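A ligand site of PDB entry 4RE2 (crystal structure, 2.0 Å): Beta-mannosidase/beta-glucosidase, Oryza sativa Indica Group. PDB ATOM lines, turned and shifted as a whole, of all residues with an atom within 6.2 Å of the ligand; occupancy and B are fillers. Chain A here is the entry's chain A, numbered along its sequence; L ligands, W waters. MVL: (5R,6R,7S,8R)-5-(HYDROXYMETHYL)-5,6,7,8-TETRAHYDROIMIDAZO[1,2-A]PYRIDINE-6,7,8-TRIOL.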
ATOM      1  N   SER A  49      11.817  22.115  23.022  1.00  0.00           N
ATOM      2  CA  SER A  49      13.157  21.647  22.662  1.00  0.00           C
ATOM      3  C   SER A  49      14.213  22.697  22.976  1.00  0.00           C
ATOM      4  O   SER A  49      13.893  23.884  23.090  1.00  0.00           O
ATOM      5  CB  SER A  49      13.225  21.221  21.198  1.00  0.00           C
ATOM      6  OG  SER A  49      13.393  22.331  20.345  1.00  0.00           O
ATOM      7  N   GLN A  52      14.733  25.642  20.530  1.00  0.00           N
ATOM      8  CA  GLN A  52      13.527  26.434  20.316  1.00  0.00           C
ATOM      9  C   GLN A  52      13.224  27.349  21.503  1.00  0.00           C
ATOM     10  O   GLN A  52      12.550  28.362  21.327  1.00  0.00           O
ATOM     11  CB  GLN A  52      12.339  25.527  19.974  1.00  0.00           C
ATOM     12  CG  GLN A  52      12.447  24.896  18.587  1.00  0.00           C
ATOM     13  CD  GLN A  52      11.307  23.961  18.301  1.00  0.00           C
ATOM     14  OE1 GLN A  52      11.325  22.797  18.707  1.00  0.00           O
ATOM     15  NE2 GLN A  52      10.295  24.458  17.607  1.00  0.00           N
ATOM     16  N   ARG A 109       8.564  17.590  28.927  1.00  0.00           N
ATOM     17  CA  ARG A 109       9.552  17.020  28.027  1.00  0.00           C
ATOM     18  C   ARG A 109      10.387  18.132  27.422  1.00  0.00           C
ATOM     19  O   ARG A 109       9.894  18.961  26.667  1.00  0.00           O
ATOM     20  CB  ARG A 109       8.933  16.089  26.967  1.00  0.00           C
ATOM     21  CG  ARG A 109       9.975  15.361  26.098  1.00  0.00           C
ATOM     22  CD  ARG A 109      10.170  16.019  24.722  1.00  0.00           C
ATOM     23  NE  ARG A 109       8.998  15.793  23.873  1.00  0.00           N
ATOM     24  CZ  ARG A 109       8.952  15.993  22.554  1.00  0.00           C
ATOM     25  NH1 ARG A 109      10.001  16.471  21.900  1.00  0.00           N
ATOM     26  NH2 ARG A 109       7.836  15.739  21.892  1.00  0.00           N
ATOM     27  N   HIS A 153      16.971  17.016  19.194  1.00  0.00           N
ATOM     28  CA  HIS A 153      15.877  17.689  18.493  1.00  0.00           C
ATOM     29  C   HIS A 153      16.481  18.626  17.443  1.00  0.00           C
ATOM     30  O   HIS A 153      16.465  19.862  17.580  1.00  0.00           O
ATOM     31  CB  HIS A 153      14.984  18.451  19.501  1.00  0.00           C
ATOM     32  CG  HIS A 153      13.589  18.745  19.002  1.00  0.00           C
ATOM     33  ND1 HIS A 153      12.461  18.490  19.760  1.00  0.00           N
ATOM     34  CD2 HIS A 153      13.145  19.277  17.834  1.00  0.00           C
ATOM     35  CE1 HIS A 153      11.394  18.886  19.092  1.00  0.00           C
ATOM     36  NE2 HIS A 153      11.773  19.345  17.915  1.00  0.00           N
ATOM     37  N   TYR A 154      17.066  18.005  16.402  1.00  0.00           N
ATOM     38  CA  TYR A 154      17.528  18.676  15.177  1.00  0.00           C
ATOM     39  C   TYR A 154      18.882  19.389  15.287  1.00  0.00           C
ATOM     40  O   TYR A 154      19.365  19.942  14.296  1.00  0.00           O
ATOM     41  CB  TYR A 154      16.473  19.645  14.608  1.00  0.00           C
ATOM     42  CG  TYR A 154      15.068  19.067  14.413  1.00  0.00           C
ATOM     43  CD1 TYR A 154      14.002  19.916  14.134  1.00  0.00           C
ATOM     44  CD2 TYR A 154      14.822  17.696  14.515  1.00  0.00           C
ATOM     45  CE1 TYR A 154      12.711  19.414  13.950  1.00  0.00           C
ATOM     46  CE2 TYR A 154      13.539  17.188  14.340  1.00  0.00           C
ATOM     47  CZ  TYR A 154      12.496  18.039  14.062  1.00  0.00           C
ATOM     48  OH  TYR A 154      11.236  17.533  13.889  1.00  0.00           O
ATOM     49  N   ASN A 198      13.787  13.145  18.661  1.00  0.00           N
ATOM     50  CA  ASN A 198      12.525  13.732  18.194  1.00  0.00           C
ATOM     51  C   ASN A 198      12.430  13.649  16.669  1.00  0.00           C
ATOM     52  O   ASN A 198      13.203  14.291  15.957  1.00  0.00           O
ATOM     53  CB  ASN A 198      12.372  15.189  18.624  1.00  0.00           C
ATOM     54  CG  ASN A 198      11.034  15.789  18.202  1.00  0.00           C
ATOM     55  OD1 ASN A 198      10.049  15.639  18.905  1.00  0.00           O
ATOM     56  ND2 ASN A 198      11.004  16.451  17.052  1.00  0.00           N
ATOM     57  N   GLU A 199      11.467  12.850  16.187  1.00  0.00           N
ATOM     58  CA  GLU A 199      11.128  12.805  14.760  1.00  0.00           C
ATOM     59  C   GLU A 199      12.295  12.546  13.802  1.00  0.00           C
ATOM     60  O   GLU A 199      12.614  13.393  12.946  1.00  0.00           O
ATOM     61  CB  GLU A 199      10.353  14.057  14.365  1.00  0.00           C
ATOM     62  CG  GLU A 199       9.104  14.198  15.235  1.00  0.00           C
ATOM     63  CD  GLU A 199       8.240  15.381  14.868  1.00  0.00           C
ATOM     64  OE1 GLU A 199       8.610  16.123  13.934  1.00  0.00           O
ATOM     65  OE2 GLU A 199       7.198  15.546  15.528  1.00  0.00           O
ATOM     66  N   HIS A 213      15.165  21.749   6.243  1.00  0.00           N
ATOM     67  CA  HIS A 213      15.826  21.899   7.532  1.00  0.00           C
ATOM     68  C   HIS A 213      17.319  21.685   7.398  1.00  0.00           C
ATOM     69  O   HIS A 213      17.777  21.147   6.392  1.00  0.00           O
ATOM     70  CB  HIS A 213      15.253  20.916   8.571  1.00  0.00           C
ATOM     71  CG  HIS A 213      13.928  21.357   9.127  1.00  0.00           C
ATOM     72  ND1 HIS A 213      13.396  20.814  10.282  1.00  0.00           N
ATOM     73  CD2 HIS A 213      13.058  22.300   8.705  1.00  0.00           C
ATOM     74  CE1 HIS A 213      12.239  21.399  10.531  1.00  0.00           C
ATOM     75  NE2 HIS A 213      12.005  22.299   9.596  1.00  0.00           N
ATOM     76  N   ASP A 266       6.839  11.107  14.644  1.00  0.00           N
ATOM     77  CA  ASP A 266       5.702  11.812  14.105  1.00  0.00           C
ATOM     78  C   ASP A 266       4.855  10.852  13.293  1.00  0.00           C
ATOM     79  O   ASP A 266       5.358   9.939  12.633  1.00  0.00           O
ATOM     80  CB  ASP A 266       6.128  13.015  13.252  1.00  0.00           C
ATOM     81  CG  ASP A 266       7.133  12.652  12.173  1.00  0.00           C
ATOM     82  OD1 ASP A 266       8.267  12.207  12.500  1.00  0.00           O
ATOM     83  OD2 ASP A 266       6.795  12.843  10.976  1.00  0.00           O
ATOM     84  N   ASN A 336       4.007  11.639  18.138  1.00  0.00           N
ATOM     85  CA  ASN A 336       3.741  13.071  17.945  1.00  0.00           C
ATOM     86  C   ASN A 336       2.666  13.199  16.866  1.00  0.00           C
ATOM     87  O   ASN A 336       2.932  12.912  15.711  1.00  0.00           O
ATOM     88  CB  ASN A 336       5.030  13.804  17.511  1.00  0.00           C
ATOM     89  CG  ASN A 336       6.113  13.832  18.600  1.00  0.00           C
ATOM     90  OD1 ASN A 336       5.884  13.471  19.755  1.00  0.00           O
ATOM     91  ND2 ASN A 336       7.293  14.317  18.235  1.00  0.00           N
ATOM     92  N   TYR A 338      -0.609  15.496  15.146  1.00  0.00           N
ATOM     93  CA  TYR A 338      -1.217  16.815  14.965  1.00  0.00           C
ATOM     94  C   TYR A 338      -2.352  16.807  13.958  1.00  0.00           C
ATOM     95  O   TYR A 338      -3.291  17.567  14.127  1.00  0.00           O
ATOM     96  CB  TYR A 338      -0.185  17.813  14.448  1.00  0.00           C
ATOM     97  CG  TYR A 338       0.911  18.183  15.420  1.00  0.00           C
ATOM     98  CD1 TYR A 338       2.027  17.369  15.593  1.00  0.00           C
ATOM     99  CD2 TYR A 338       0.846  19.387  16.142  1.00  0.00           C
ATOM    100  CE1 TYR A 338       3.040  17.725  16.489  1.00  0.00           C
ATOM    101  CE2 TYR A 338       1.853  19.774  17.010  1.00  0.00           C
ATOM    102  CZ  TYR A 338       2.939  18.937  17.184  1.00  0.00           C
ATOM    103  OH  TYR A 338       3.933  19.325  18.055  1.00  0.00           O
ATOM    104  N   SER A 379      -0.013  26.967  10.347  1.00  0.00           N
ATOM    105  CA  SER A 379       0.954  26.187   9.573  1.00  0.00           C
ATOM    106  C   SER A 379       0.313  25.542   8.342  1.00  0.00           C
ATOM    107  O   SER A 379      -0.778  24.976   8.444  1.00  0.00           O
ATOM    108  CB  SER A 379       1.580  25.088  10.443  1.00  0.00           C
ATOM    109  OG  SER A 379       2.581  25.609  11.295  1.00  0.00           O
ATOM    110  N   TRP A 381       0.818  22.889   6.825  1.00  0.00           N
ATOM    111  CA  TRP A 381       0.646  21.438   6.880  1.00  0.00           C
ATOM    112  C   TRP A 381      -0.451  21.008   7.863  1.00  0.00           C
ATOM    113  O   TRP A 381      -0.857  19.837   7.870  1.00  0.00           O
ATOM    114  CB  TRP A 381       1.980  20.754   7.229  1.00  0.00           C
ATOM    115  CG  TRP A 381       2.583  21.232   8.509  1.00  0.00           C
ATOM    116  CD1 TRP A 381       3.498  22.237   8.656  1.00  0.00           C
ATOM    117  CD2 TRP A 381       2.317  20.745   9.837  1.00  0.00           C
ATOM    118  NE1 TRP A 381       3.805  22.414   9.986  1.00  0.00           N
ATOM    119  CE2 TRP A 381       3.089  21.518  10.730  1.00  0.00           C
ATOM    120  CE3 TRP A 381       1.488  19.738  10.356  1.00  0.00           C
ATOM    121  CZ2 TRP A 381       3.092  21.298  12.115  1.00  0.00           C
ATOM    122  CZ3 TRP A 381       1.467  19.535  11.732  1.00  0.00           C
ATOM    123  CH2 TRP A 381       2.269  20.308  12.594  1.00  0.00           C
ATOM    124  N   GLU A 409       3.254  14.690  21.577  1.00  0.00           N
ATOM    125  CA  GLU A 409       3.035  16.069  21.119  1.00  0.00           C
ATOM    126  C   GLU A 409       1.663  16.181  20.488  1.00  0.00           C
ATOM    127  O   GLU A 409       1.230  15.274  19.798  1.00  0.00           O
ATOM    128  CB  GLU A 409       4.036  16.496  20.034  1.00  0.00           C
ATOM    129  CG  GLU A 409       5.425  16.822  20.513  1.00  0.00           C
ATOM    130  CD  GLU A 409       6.323  17.278  19.386  1.00  0.00           C
ATOM    131  OE1 GLU A 409       5.788  17.701  18.310  1.00  0.00           O
ATOM    132  OE2 GLU A 409       7.539  17.224  19.573  1.00  0.00           O
ATOM    133  N   TRP A 456       2.155  20.328  22.670  1.00  0.00           N
ATOM    134  CA  TRP A 456       3.149  21.245  22.094  1.00  0.00           C
ATOM    135  C   TRP A 456       2.471  22.617  21.947  1.00  0.00           C
ATOM    136  O   TRP A 456       1.550  22.746  21.161  1.00  0.00           O
ATOM    137  CB  TRP A 456       3.633  20.771  20.715  1.00  0.00           C
ATOM    138  CG  TRP A 456       4.769  21.656  20.221  1.00  0.00           C
ATOM    139  CD1 TRP A 456       4.666  22.863  19.565  1.00  0.00           C
ATOM    140  CD2 TRP A 456       6.162  21.421  20.419  1.00  0.00           C
ATOM    141  NE1 TRP A 456       5.923  23.388  19.338  1.00  0.00           N
ATOM    142  CE2 TRP A 456       6.860  22.520  19.853  1.00  0.00           C
ATOM    143  CE3 TRP A 456       6.889  20.381  21.019  1.00  0.00           C
ATOM    144  CZ2 TRP A 456       8.252  22.601  19.869  1.00  0.00           C
ATOM    145  CZ3 TRP A 456       8.286  20.459  21.028  1.00  0.00           C
ATOM    146  CH2 TRP A 456       8.942  21.568  20.467  1.00  0.00           C
ATOM    147  N   ASN A 461       7.327  29.951  20.622  1.00  0.00           N
ATOM    148  CA  ASN A 461       8.776  29.818  20.504  1.00  0.00           C
ATOM    149  C   ASN A 461       9.293  29.855  19.072  1.00  0.00           C
ATOM    150  O   ASN A 461       8.546  30.127  18.135  1.00  0.00           O
ATOM    151  CB  ASN A 461       9.290  28.579  21.287  1.00  0.00           C
ATOM    152  CG  ASN A 461       8.708  27.278  20.793  1.00  0.00           C
ATOM    153  OD1 ASN A 461       8.786  26.949  19.616  1.00  0.00           O
ATOM    154  ND2 ASN A 461       8.133  26.502  21.728  1.00  0.00           N
ATOM    155  N   PHE A 462      10.585  29.599  18.917  1.00  0.00           N
ATOM    156  CA  PHE A 462      11.224  29.638  17.605  1.00  0.00           C
ATOM    157  C   PHE A 462      10.770  28.414  16.804  1.00  0.00           C
ATOM    158  O   PHE A 462      11.171  27.293  17.099  1.00  0.00           O
ATOM    159  CB  PHE A 462      12.742  29.700  17.764  1.00  0.00           C
ATOM    160  CG  PHE A 462      13.497  29.592  16.471  1.00  0.00           C
ATOM    161  CD1 PHE A 462      13.647  30.696  15.632  1.00  0.00           C
ATOM    162  CD2 PHE A 462      14.091  28.380  16.097  1.00  0.00           C
ATOM    163  CE1 PHE A 462      14.367  30.604  14.435  1.00  0.00           C
ATOM    164  CE2 PHE A 462      14.798  28.269  14.911  1.00  0.00           C
ATOM    165  CZ  PHE A 462      14.942  29.395  14.073  1.00  0.00           C
ATOM    166  N   GLU A 463       9.943  28.654  15.774  1.00  0.00           N
ATOM    167  CA  GLU A 463       9.322  27.574  14.983  1.00  0.00           C
ATOM    168  C   GLU A 463      10.120  27.213  13.725  1.00  0.00           C
ATOM    169  O   GLU A 463       9.613  27.262  12.605  1.00  0.00           O
ATOM    170  CB  GLU A 463       7.857  27.933  14.678  1.00  0.00           C
ATOM    171  CG  GLU A 463       7.048  26.924  13.847  1.00  0.00           C
ATOM    172  CD  GLU A 463       7.079  25.487  14.351  1.00  0.00           C
ATOM    173  OE1 GLU A 463       7.336  25.249  15.549  1.00  0.00           O
ATOM    174  OE2 GLU A 463       6.818  24.587  13.522  1.00  0.00           O
ATOM    175  N   TRP A 464      11.376  26.838  13.944  1.00  0.00           N
ATOM    176  CA  TRP A 464      12.283  26.404  12.888  1.00  0.00           C
ATOM    177  C   TRP A 464      12.217  27.326  11.667  1.00  0.00           C
ATOM    178  O   TRP A 464      12.470  28.528  11.810  1.00  0.00           O
ATOM    179  CB  TRP A 464      12.053  24.904  12.568  1.00  0.00           C
ATOM    180  CG  TRP A 464      12.272  24.023  13.789  1.00  0.00           C
ATOM    181  CD1 TRP A 464      11.324  23.296  14.477  1.00  0.00           C
ATOM    182  CD2 TRP A 464      13.513  23.824  14.489  1.00  0.00           C
ATOM    183  NE1 TRP A 464      11.914  22.632  15.540  1.00  0.00           N
ATOM    184  CE2 TRP A 464      13.251  22.953  15.569  1.00  0.00           C
ATOM    185  CE3 TRP A 464      14.821  24.294  14.304  1.00  0.00           C
ATOM    186  CZ2 TRP A 464      14.237  22.534  16.456  1.00  0.00           C
ATOM    187  CZ3 TRP A 464      15.811  23.890  15.175  1.00  0.00           C
ATOM    188  CH2 TRP A 464      15.519  23.015  16.249  1.00  0.00           C
ATOM    189  N   SER A 470       4.908  31.927  13.738  1.00  0.00           N
ATOM    190  CA  SER A 470       3.994  30.858  14.147  1.00  0.00           C
ATOM    191  C   SER A 470       4.036  30.728  15.665  1.00  0.00           C
ATOM    192  O   SER A 470       5.102  30.604  16.256  1.00  0.00           O
ATOM    193  CB  SER A 470       4.442  29.545  13.497  1.00  0.00           C
ATOM    194  OG  SER A 470       3.988  28.430  14.248  1.00  0.00           O
ATOM    195  N   PHE A 472       2.716  28.458  18.708  1.00  0.00           N
ATOM    196  CA  PHE A 472       2.164  27.153  19.147  1.00  0.00           C
ATOM    197  C   PHE A 472       1.843  27.072  20.653  1.00  0.00           C
ATOM    198  O   PHE A 472       1.333  26.050  21.141  1.00  0.00           O
ATOM    199  CB  PHE A 472       3.142  26.006  18.795  1.00  0.00           C
ATOM    200  CG  PHE A 472       2.957  25.417  17.421  1.00  0.00           C
ATOM    201  CD1 PHE A 472       2.056  24.357  17.217  1.00  0.00           C
ATOM    202  CD2 PHE A 472       3.674  25.907  16.323  1.00  0.00           C
ATOM    203  CE1 PHE A 472       1.867  23.813  15.951  1.00  0.00           C
ATOM    204  CE2 PHE A 472       3.503  25.369  15.042  1.00  0.00           C
ATOM    205  CZ  PHE A 472       2.598  24.302  14.849  1.00  0.00           C
HETATM  206  C1  MVL L   1       6.903  19.169  16.107  1.00  0.00           C
HETATM  207  N10 MVL L   1       6.113  20.141  15.717  1.00  0.00           N
HETATM  208  C3  MVL L   1       8.701  20.718  16.840  1.00  0.00           C
HETATM  209  C4  MVL L   1       7.812  21.781  16.159  1.00  0.00           C
HETATM  210  C5  MVL L   1       6.314  21.492  16.312  1.00  0.00           C
HETATM  211  C6  MVL L   1       5.391  22.539  15.678  1.00  0.00           C
HETATM  212  C7  MVL L   1       5.547  18.335  14.601  1.00  0.00           C
HETATM  213  C8  MVL L   1       5.262  19.680  14.780  1.00  0.00           C
HETATM  214  N1  MVL L   1       6.565  18.043  15.449  1.00  0.00           N
HETATM  215  O3  MVL L   1       9.811  20.403  15.990  1.00  0.00           O
HETATM  216  O2  MVL L   1       8.810  18.277  17.289  1.00  0.00           O
HETATM  217  O4  MVL L   1       8.139  23.060  16.715  1.00  0.00           O
HETATM  218  C2  MVL L   1       7.946  19.415  17.153  1.00  0.00           C
HETATM  219  O6  MVL L   1       5.520  22.538  14.262  1.00  0.00           O
HETATM  220  O   HOH W   1       9.221  19.073  13.771  1.00  0.00           O
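The side-chain carboxylate of Glu 409 lies within hydrogen-bond range of the side-chain amide nitrogen of Asn 336, at 3.2 Å.
The side-chain hydroxyl of Tyr 154 is in hydrogen-bond range of the side-chain carboxylate of Glu 199, at 3.0 Å.
NE2 of Gln 52 lies close to NE1 of Trp 464, at 3.2 Å.
ND2 of Asn 198 lies within hydrogen-bond range of NE2 of His 153.
OD1 of Asn 198 sits at hydrogen-bond distance from ND2 of Asn 336.
NH1 of Arg 109 is in hydrogen-bond range of OD1 of Asn 198.
The side-chain amide oxygen (OD1) of Asn 198 lies close to the side-chain carboxylate (OE2) of Glu 409, 3.0 Å away.
The side-chain amide nitrogen (ND2) of Asn 198 is in hydrogen-bond range of the side-chain hydroxyl (OH) of Tyr 154, 3.4 Å away.
Water W1 lies within hydrogen-bond range of OH of Tyr 154 (2.5 Å), O3 of the ligand (2.7 Å) and OE1 of Glu 199 (3.0 Å).
N10 of the ligand lies close to OH of Tyr 338 (3.3 Å).
Tyr 154 touches the ligand (CE1 to O3, 3.7 Å).
Trp 381 touches the ligand (CZ2 to O6, 3.5 Å).
Phe 472 touches the ligand (CZ to C6, 3.4 Å).
Hydrophobic or aromatic side chains within 4 Å of the ligand: His 153, Tyr 154, Tyr 338, Trp 381, Trp 456, Trp 464 and Phe 472.
Within 4 Å of the ligand: Gln 52, His 153, Tyr 154, Asn 198, Glu 199, Tyr 338, Trp 381, Glu 409, Trp 456, Glu 463, Trp 464 and Phe 472.
The nearest printed residue that does not touch the ligand is Asn 336 (4.3 Å).
The indole nitrogen (NE1) of Trp 464 sits at hydrogen-bond distance from an oxygen (O3) of the ligand (3.1 Å).
O2 of the ligand is in hydrogen-bond range of ND2 of Asn 198, 2.9 Å away.
The indole nitrogen (NE1) of Trp 456 lies close to an oxygen (O4) of the ligand (3.4 Å).
The side-chain carboxylate (OE2) of Glu 409 sits at hydrogen-bond distance from an oxygen (O2) of the ligand, 2.8 Å away.
OE2 of Glu 463 lies within hydrogen-bond range of O6 of the ligand.
O4 of the ligand lies within hydrogen-bond range of NE2 of Gln 52, 2.7 Å away.
An oxygen (O3) of the ligand lies within hydrogen-bond range of a ring nitrogen (NE2) of His 153, 2.9 Å away.
The side-chain carboxylate of Glu 199 sits at hydrogen-bond distance from a nitrogen (N1) of the ligand.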
